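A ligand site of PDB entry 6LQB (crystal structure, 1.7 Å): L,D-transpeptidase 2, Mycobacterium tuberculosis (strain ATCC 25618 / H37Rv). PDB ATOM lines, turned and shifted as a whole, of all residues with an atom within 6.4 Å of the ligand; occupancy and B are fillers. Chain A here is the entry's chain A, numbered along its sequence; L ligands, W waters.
The backbone NH of Cys 215 is in hydrogen-bond range of an oxygen (O2) of the ligand (3.1 Å).
The side-chain sulfur (SG) of Cys 215 is bonded to a carbon (C6) of the ligand, 1.8 Å away.
The backbone carbonyl oxygen of Tyr 169 sits close to an oxygen (O6) of the ligand, 2.6 Å away.
The side-chain hydroxyl (OH) of Tyr 169 lies close to a sulfur (S1) of the ligand.
The side-chain hydroxyl (OH) of Tyr 179 sits close to an oxygen (O4) of the ligand (3.2 Å).
The side-chain sulfur (SG) of Cys 215 sits at hydrogen-bond distance from the backbone NH (N) of Phe 195 (3.6 Å).
The side-chain hydroxyl (OG) of Ser 212 lies within hydrogen-bond range of the backbone carbonyl oxygen (O) of Cys 215, at 2.8 Å.
OH of Tyr 169 is in hydrogen-bond range of O of Ser 192 (3.2 Å).
The backbone carbonyl oxygen of Thr 181 lies within hydrogen-bond range of the backbone NH of Met 164 (2.9 Å).
The backbone NH (N) of Gly 214 sits at hydrogen-bond distance from the side-chain hydroxyl (OG) of Ser 212 (2.7 Å).
Residues that only touch the ligand: Met 164, Ser 192, Gly 193, His 213 and Gly 214.
Hydrophobic or aromatic side chains within 4 Å of the ligand: Met 164, Tyr 169, Tyr 179 and His 213.
Within 4 Å of the ligand: Met 164, Tyr 169, Tyr 179, Ser 192, Gly 193, His 213, Gly 214 and Cys 215.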
ATOM      1  N   THR A 146      21.606 -20.578  -4.548  1.00  0.00           N
ATOM      2  CA  THR A 146      20.576 -20.754  -3.525  1.00  0.00           C
ATOM      3  C   THR A 146      19.402 -21.455  -4.174  1.00  0.00           C
ATOM      4  O   THR A 146      18.315 -20.881  -4.309  1.00  0.00           O
ATOM      5  CB  THR A 146      20.159 -19.401  -2.942  1.00  0.00           C
ATOM      6  OG1 THR A 146      19.664 -18.561  -3.997  1.00  0.00           O
ATOM      7  CG2 THR A 146      21.343 -18.716  -2.272  1.00  0.00           C
ATOM      8  N   MET A 164       9.136 -11.087   5.181  1.00  0.00           N
ATOM      9  CA  MET A 164      10.318 -11.947   5.264  1.00  0.00           C
ATOM     10  C   MET A 164      11.429 -11.066   5.822  1.00  0.00           C
ATOM     11  O   MET A 164      11.764 -10.033   5.234  1.00  0.00           O
ATOM     12  CB  MET A 164      10.712 -12.485   3.887  1.00  0.00           C
ATOM     13  CG  MET A 164       9.605 -13.096   3.016  1.00  0.00           C
ATOM     14  SD  MET A 164       8.671 -14.478   3.715  1.00  0.00           S
ATOM     15  CE  MET A 164       7.684 -15.003   2.308  1.00  0.00           C
ATOM     16  N   ASP A 165      12.002 -11.468   6.958  1.00  0.00           N
ATOM     17  CA  ASP A 165      12.881 -10.585   7.718  1.00  0.00           C
ATOM     18  C   ASP A 165      14.138 -11.355   8.097  1.00  0.00           C
ATOM     19  O   ASP A 165      14.075 -12.405   8.738  1.00  0.00           O
ATOM     20  CB  ASP A 165      12.185 -10.036   8.967  1.00  0.00           C
ATOM     21  CG  ASP A 165      12.908  -8.828   9.544  1.00  0.00           C
ATOM     22  OD1 ASP A 165      14.149  -8.831   9.546  1.00  0.00           O
ATOM     23  OD2 ASP A 165      12.229  -7.872   9.978  1.00  0.00           O
ATOM     24  N   TYR A 169      16.860 -15.152  10.663  1.00  0.00           N
ATOM     25  CA  TYR A 169      17.940 -16.087  10.378  1.00  0.00           C
ATOM     26  C   TYR A 169      19.283 -15.592  10.884  1.00  0.00           C
ATOM     27  O   TYR A 169      20.310 -16.216  10.584  1.00  0.00           O
ATOM     28  CB  TYR A 169      18.025 -16.360   8.868  1.00  0.00           C
ATOM     29  CG  TYR A 169      16.825 -17.088   8.307  1.00  0.00           C
ATOM     30  CD1 TYR A 169      15.605 -16.445   8.165  1.00  0.00           C
ATOM     31  CD2 TYR A 169      16.916 -18.425   7.925  1.00  0.00           C
ATOM     32  CE1 TYR A 169      14.500 -17.115   7.658  1.00  0.00           C
ATOM     33  CE2 TYR A 169      15.820 -19.097   7.421  1.00  0.00           C
ATOM     34  CZ  TYR A 169      14.614 -18.444   7.281  1.00  0.00           C
ATOM     35  OH  TYR A 169      13.522 -19.102   6.775  1.00  0.00           O
ATOM     36  N   GLY A 170      19.298 -14.507  11.652  1.00  0.00           N
ATOM     37  CA  GLY A 170      20.496 -14.035  12.307  1.00  0.00           C
ATOM     38  C   GLY A 170      21.157 -12.861  11.606  1.00  0.00           C
ATOM     39  O   GLY A 170      22.118 -12.301  12.130  1.00  0.00           O
ATOM     40  N   VAL A 171      20.646 -12.481  10.433  1.00  0.00           N
ATOM     41  CA  VAL A 171      21.241 -11.466   9.579  1.00  0.00           C
ATOM     42  C   VAL A 171      20.483 -10.153   9.787  1.00  0.00           C
ATOM     43  O   VAL A 171      19.279 -10.099   9.464  1.00  0.00           O
ATOM     44  CB  VAL A 171      21.210 -11.878   8.107  1.00  0.00           C
ATOM     45  CG1 VAL A 171      21.903 -10.850   7.234  1.00  0.00           C
ATOM     46  CG2 VAL A 171      21.841 -13.260   7.928  1.00  0.00           C
ATOM     47  N   ASN A 177      23.748  -8.790   3.382  1.00  0.00           N
ATOM     48  CA  ASN A 177      22.888  -9.892   3.000  1.00  0.00           C
ATOM     49  C   ASN A 177      21.539  -9.891   3.723  1.00  0.00           C
ATOM     50  O   ASN A 177      20.818 -10.891   3.653  1.00  0.00           O
ATOM     51  CB  ASN A 177      23.596 -11.224   3.238  1.00  0.00           C
ATOM     52  CG  ASN A 177      24.594 -11.551   2.139  1.00  0.00           C
ATOM     53  OD1 ASN A 177      24.416 -11.166   0.986  1.00  0.00           O
ATOM     54  ND2 ASN A 177      25.638 -12.289   2.495  1.00  0.00           N
ATOM     55  N   TYR A 179      17.572  -8.493   4.650  1.00  0.00           N
ATOM     56  CA  TYR A 179      16.425  -8.011   3.886  1.00  0.00           C
ATOM     57  C   TYR A 179      15.218  -7.930   4.800  1.00  0.00           C
ATOM     58  O   TYR A 179      15.088  -8.695   5.764  1.00  0.00           O
ATOM     59  CB  TYR A 179      16.128  -8.896   2.667  1.00  0.00           C
ATOM     60  CG  TYR A 179      15.880 -10.354   2.989  1.00  0.00           C
ATOM     61  CD1 TYR A 179      14.708 -10.758   3.617  1.00  0.00           C
ATOM     62  CD2 TYR A 179      16.807 -11.330   2.645  1.00  0.00           C
ATOM     63  CE1 TYR A 179      14.474 -12.082   3.909  1.00  0.00           C
ATOM     64  CE2 TYR A 179      16.582 -12.664   2.934  1.00  0.00           C
ATOM     65  CZ  TYR A 179      15.408 -13.031   3.562  1.00  0.00           C
ATOM     66  OH  TYR A 179      15.174 -14.355   3.854  1.00  0.00           O
ATOM     67  N   THR A 181      11.315  -7.716   3.600  1.00  0.00           N
ATOM     68  CA  THR A 181      10.606  -7.828   2.337  1.00  0.00           C
ATOM     69  C   THR A 181       9.124  -8.037   2.590  1.00  0.00           C
ATOM     70  O   THR A 181       8.737  -9.017   3.243  1.00  0.00           O
ATOM     71  CB  THR A 181      11.160  -9.009   1.520  1.00  0.00           C
ATOM     72  OG1 THR A 181      12.574  -8.879   1.375  1.00  0.00           O
ATOM     73  CG2 THR A 181      10.491  -9.098   0.159  1.00  0.00           C
ATOM     74  N   VAL A 183       5.694  -9.335   1.220  1.00  0.00           N
ATOM     75  CA  VAL A 183       5.308 -10.331   0.236  1.00  0.00           C
ATOM     76  C   VAL A 183       3.804 -10.559   0.314  1.00  0.00           C
ATOM     77  O   VAL A 183       3.254 -10.785   1.396  1.00  0.00           O
ATOM     78  CB  VAL A 183       6.082 -11.648   0.454  1.00  0.00           C
ATOM     79  CG1 VAL A 183       5.550 -12.726  -0.452  1.00  0.00           C
ATOM     80  CG2 VAL A 183       7.573 -11.421   0.192  1.00  0.00           C
ATOM     81  N   SER A 192      11.424 -24.743   6.196  1.00  0.00           N
ATOM     82  CA  SER A 192      12.665 -24.033   5.926  1.00  0.00           C
ATOM     83  C   SER A 192      12.434 -22.654   5.316  1.00  0.00           C
ATOM     84  O   SER A 192      13.378 -21.862   5.243  1.00  0.00           O
ATOM     85  CB  SER A 192      13.587 -24.865   5.037  1.00  0.00           C
ATOM     86  OG  SER A 192      13.116 -24.952   3.703  1.00  0.00           O
ATOM     87  N   GLY A 193      11.234 -22.380   4.831  1.00  0.00           N
ATOM     88  CA  GLY A 193      10.918 -21.040   4.376  1.00  0.00           C
ATOM     89  C   GLY A 193      10.587 -20.894   2.911  1.00  0.00           C
ATOM     90  O   GLY A 193      10.511 -19.773   2.410  1.00  0.00           O
ATOM     91  N   VAL A 194      10.400 -21.997   2.185  1.00  0.00           N
ATOM     92  CA  VAL A 194      10.001 -21.890   0.790  1.00  0.00           C
ATOM     93  C   VAL A 194       8.521 -21.553   0.729  1.00  0.00           C
ATOM     94  O   VAL A 194       7.697 -22.184   1.405  1.00  0.00           O
ATOM     95  CB  VAL A 194      10.306 -23.197   0.030  1.00  0.00           C
ATOM     96  CG1 VAL A 194       9.833 -23.073  -1.420  1.00  0.00           C
ATOM     97  CG2 VAL A 194      11.802 -23.483   0.056  1.00  0.00           C
ATOM     98  N   PHE A 195       8.188 -20.516  -0.040  1.00  0.00           N
ATOM     99  CA  PHE A 195       6.824 -20.120  -0.333  1.00  0.00           C
ATOM    100  C   PHE A 195       6.635 -20.021  -1.838  1.00  0.00           C
ATOM    101  O   PHE A 195       7.570 -19.676  -2.583  1.00  0.00           O
ATOM    102  CB  PHE A 195       6.446 -18.743   0.250  1.00  0.00           C
ATOM    103  CG  PHE A 195       6.361 -18.694   1.744  1.00  0.00           C
ATOM    104  CD1 PHE A 195       7.513 -18.627   2.508  1.00  0.00           C
ATOM    105  CD2 PHE A 195       5.128 -18.626   2.375  1.00  0.00           C
ATOM    106  CE1 PHE A 195       7.423 -18.549   3.912  1.00  0.00           C
ATOM    107  CE2 PHE A 195       5.041 -18.530   3.754  1.00  0.00           C
ATOM    108  CZ  PHE A 195       6.193 -18.500   4.518  1.00  0.00           C
ATOM    109  N   HIS A 197       4.767 -17.331  -4.001  1.00  0.00           N
ATOM    110  CA  HIS A 197       4.287 -16.009  -3.610  1.00  0.00           C
ATOM    111  C   HIS A 197       4.388 -15.017  -4.760  1.00  0.00           C
ATOM    112  O   HIS A 197       5.052 -15.257  -5.771  1.00  0.00           O
ATOM    113  CB  HIS A 197       5.059 -15.476  -2.394  1.00  0.00           C
ATOM    114  CG  HIS A 197       6.492 -15.159  -2.675  1.00  0.00           C
ATOM    115  ND1 HIS A 197       6.890 -13.983  -3.273  1.00  0.00           N
ATOM    116  CD2 HIS A 197       7.619 -15.860  -2.436  1.00  0.00           C
ATOM    117  CE1 HIS A 197       8.200 -13.977  -3.402  1.00  0.00           C
ATOM    118  NE2 HIS A 197       8.675 -15.106  -2.896  1.00  0.00           N
ATOM    119  N   SER A 212      15.547 -16.220  -7.534  1.00  0.00           N
ATOM    120  CA  SER A 212      15.058 -16.173  -6.165  1.00  0.00           C
ATOM    121  C   SER A 212      16.109 -16.700  -5.188  1.00  0.00           C
ATOM    122  O   SER A 212      17.152 -17.248  -5.573  1.00  0.00           O
ATOM    123  CB  SER A 212      13.774 -16.979  -6.001  1.00  0.00           C
ATOM    124  OG  SER A 212      14.071 -18.310  -5.673  1.00  0.00           O
ATOM    125  N   HIS A 213      15.834 -16.563  -3.894  1.00  0.00           N
ATOM    126  CA  HIS A 213      16.613 -17.240  -2.877  1.00  0.00           C
ATOM    127  C   HIS A 213      16.156 -18.664  -2.616  1.00  0.00           C
ATOM    128  O   HIS A 213      16.675 -19.311  -1.704  1.00  0.00           O
ATOM    129  CB  HIS A 213      16.586 -16.442  -1.571  1.00  0.00           C
ATOM    130  CG  HIS A 213      17.361 -15.168  -1.636  1.00  0.00           C
ATOM    131  ND1 HIS A 213      16.781 -13.959  -1.964  1.00  0.00           N
ATOM    132  CD2 HIS A 213      18.673 -14.918  -1.422  1.00  0.00           C
ATOM    133  CE1 HIS A 213      17.712 -13.020  -1.948  1.00  0.00           C
ATOM    134  NE2 HIS A 213      18.861 -13.571  -1.627  1.00  0.00           N
ATOM    135  N   GLY A 214      15.225 -19.179  -3.417  1.00  0.00           N
ATOM    136  CA  GLY A 214      14.680 -20.495  -3.165  1.00  0.00           C
ATOM    137  C   GLY A 214      13.182 -20.517  -3.297  1.00  0.00           C
ATOM    138  O   GLY A 214      12.590 -21.564  -3.589  1.00  0.00           O
ATOM    139  N   CYS A 215      12.533 -19.384  -3.067  1.00  0.00           N
ATOM    140  CA  CYS A 215      11.089 -19.338  -3.175  1.00  0.00           C
ATOM    141  C   CYS A 215      10.654 -19.478  -4.623  1.00  0.00           C
ATOM    142  O   CYS A 215      11.422 -19.282  -5.568  1.00  0.00           O
ATOM    143  CB  CYS A 215      10.557 -18.031  -2.578  1.00  0.00           C
ATOM    144  SG  CYS A 215      10.558 -17.961  -0.778  1.00  0.00           S
ATOM    145  N   LEU A 216       9.388 -19.871  -4.796  1.00  0.00           N
ATOM    146  CA  LEU A 216       8.771 -19.993  -6.112  1.00  0.00           C
ATOM    147  C   LEU A 216       8.078 -18.680  -6.410  1.00  0.00           C
ATOM    148  O   LEU A 216       6.936 -18.449  -6.016  1.00  0.00           O
ATOM    149  CB  LEU A 216       7.795 -21.173  -6.154  1.00  0.00           C
ATOM    150  CG  LEU A 216       8.414 -22.558  -6.396  1.00  0.00           C
ATOM    151  CD1 LEU A 216       9.408 -22.870  -5.305  1.00  0.00           C
ATOM    152  CD2 LEU A 216       7.337 -23.658  -6.460  1.00  0.00           C
ATOM    153  N   ASN A 217       8.790 -17.782  -7.125  1.00  0.00           N
ATOM    154  CA  ASN A 217       8.230 -16.500  -7.550  1.00  0.00           C
ATOM    155  C   ASN A 217       7.231 -16.701  -8.671  1.00  0.00           C
ATOM    156  O   ASN A 217       7.559 -17.316  -9.693  1.00  0.00           O
ATOM    157  CB  ASN A 217       9.325 -15.576  -8.121  1.00  0.00           C
ATOM    158  CG  ASN A 217      10.279 -14.977  -7.098  1.00  0.00           C
ATOM    159  OD1 ASN A 217      11.117 -14.148  -7.470  1.00  0.00           O
ATOM    160  ND2 ASN A 217      10.208 -15.388  -5.841  1.00  0.00           N
HETATM  161  C1  LIG L   1      19.639 -20.620   3.965  1.00  0.00           C
HETATM  162  N1  LIG L   1      17.790 -22.052   5.164  1.00  0.00           N
HETATM  163  O1  LIG L   1      20.690 -20.842   3.460  1.00  0.00           O
HETATM  164  C2  LIG L   1      18.439 -21.603   3.745  1.00  0.00           C
HETATM  165  C3  LIG L   1      17.525 -21.054   3.022  1.00  0.00           C
HETATM  166  C4  LIG L   1      16.821 -21.211   5.371  1.00  0.00           C
HETATM  167  C5  LIG L   1      16.312 -20.833   3.967  1.00  0.00           C
HETATM  168  C6  LIG L   1      12.139 -17.151  -0.467  1.00  0.00           C
HETATM  169  C7  LIG L   1      12.031 -17.181   1.065  1.00  0.00           C
HETATM  170  O2  LIG L   1      13.146 -17.174  -1.039  1.00  0.00           O
HETATM  171  C8  LIG L   1      13.352 -17.433   1.820  1.00  0.00           C
HETATM  172  C9  LIG L   1      11.487 -15.852   1.617  1.00  0.00           C
HETATM  173  C10 LIG L   1      11.475 -15.941   3.143  1.00  0.00           C
HETATM  174  O3  LIG L   1      12.315 -14.799   1.228  1.00  0.00           O
HETATM  175  C11 LIG L   1      13.934 -18.934   1.785  1.00  0.00           C
HETATM  176  C12 LIG L   1      15.445 -18.687   2.117  1.00  0.00           C
HETATM  177  N2  LIG L   1      14.386 -16.685   1.385  1.00  0.00           N
HETATM  178  S1  LIG L   1      15.782 -19.136   3.904  1.00  0.00           S
HETATM  179  C13 LIG L   1      15.628 -17.332   1.902  1.00  0.00           C
HETATM  180  C14 LIG L   1      17.003 -16.685   1.765  1.00  0.00           C
HETATM  181  C15 LIG L   1      13.783 -19.628   0.541  1.00  0.00           C
HETATM  182  O4  LIG L   1      17.106 -15.442   1.600  1.00  0.00           O
HETATM  183  O5  LIG L   1      18.036 -17.399   1.821  1.00  0.00           O
HETATM  184  N3  LIG L   1      19.443 -19.444   4.782  1.00  0.00           N
HETATM  185  C16 LIG L   1      20.532 -18.502   5.008  1.00  0.00           C
HETATM  186  C17 LIG L   1      21.034 -18.326   6.288  1.00  0.00           C
HETATM  187  C18 LIG L   1      22.061 -17.417   6.509  1.00  0.00           C
HETATM  188  C19 LIG L   1      22.582 -16.698   5.451  1.00  0.00           C
HETATM  189  C20 LIG L   1      22.080 -16.874   4.171  1.00  0.00           C
HETATM  190  C21 LIG L   1      21.044 -17.780   3.946  1.00  0.00           C
HETATM  191  C22 LIG L   1      22.609 -17.227   7.920  1.00  0.00           C
HETATM  192  O6  LIG L   1      21.857 -17.414   8.921  1.00  0.00           O
HETATM  193  O7  LIG L   1      23.815 -16.889   8.101  1.00  0.00           O
HETATM  194  O   HOH W   1      17.014 -24.716   6.762  1.00  0.00           O
HETATM  195  O   HOH W   2      15.857 -22.952   0.722  1.00  0.00           O
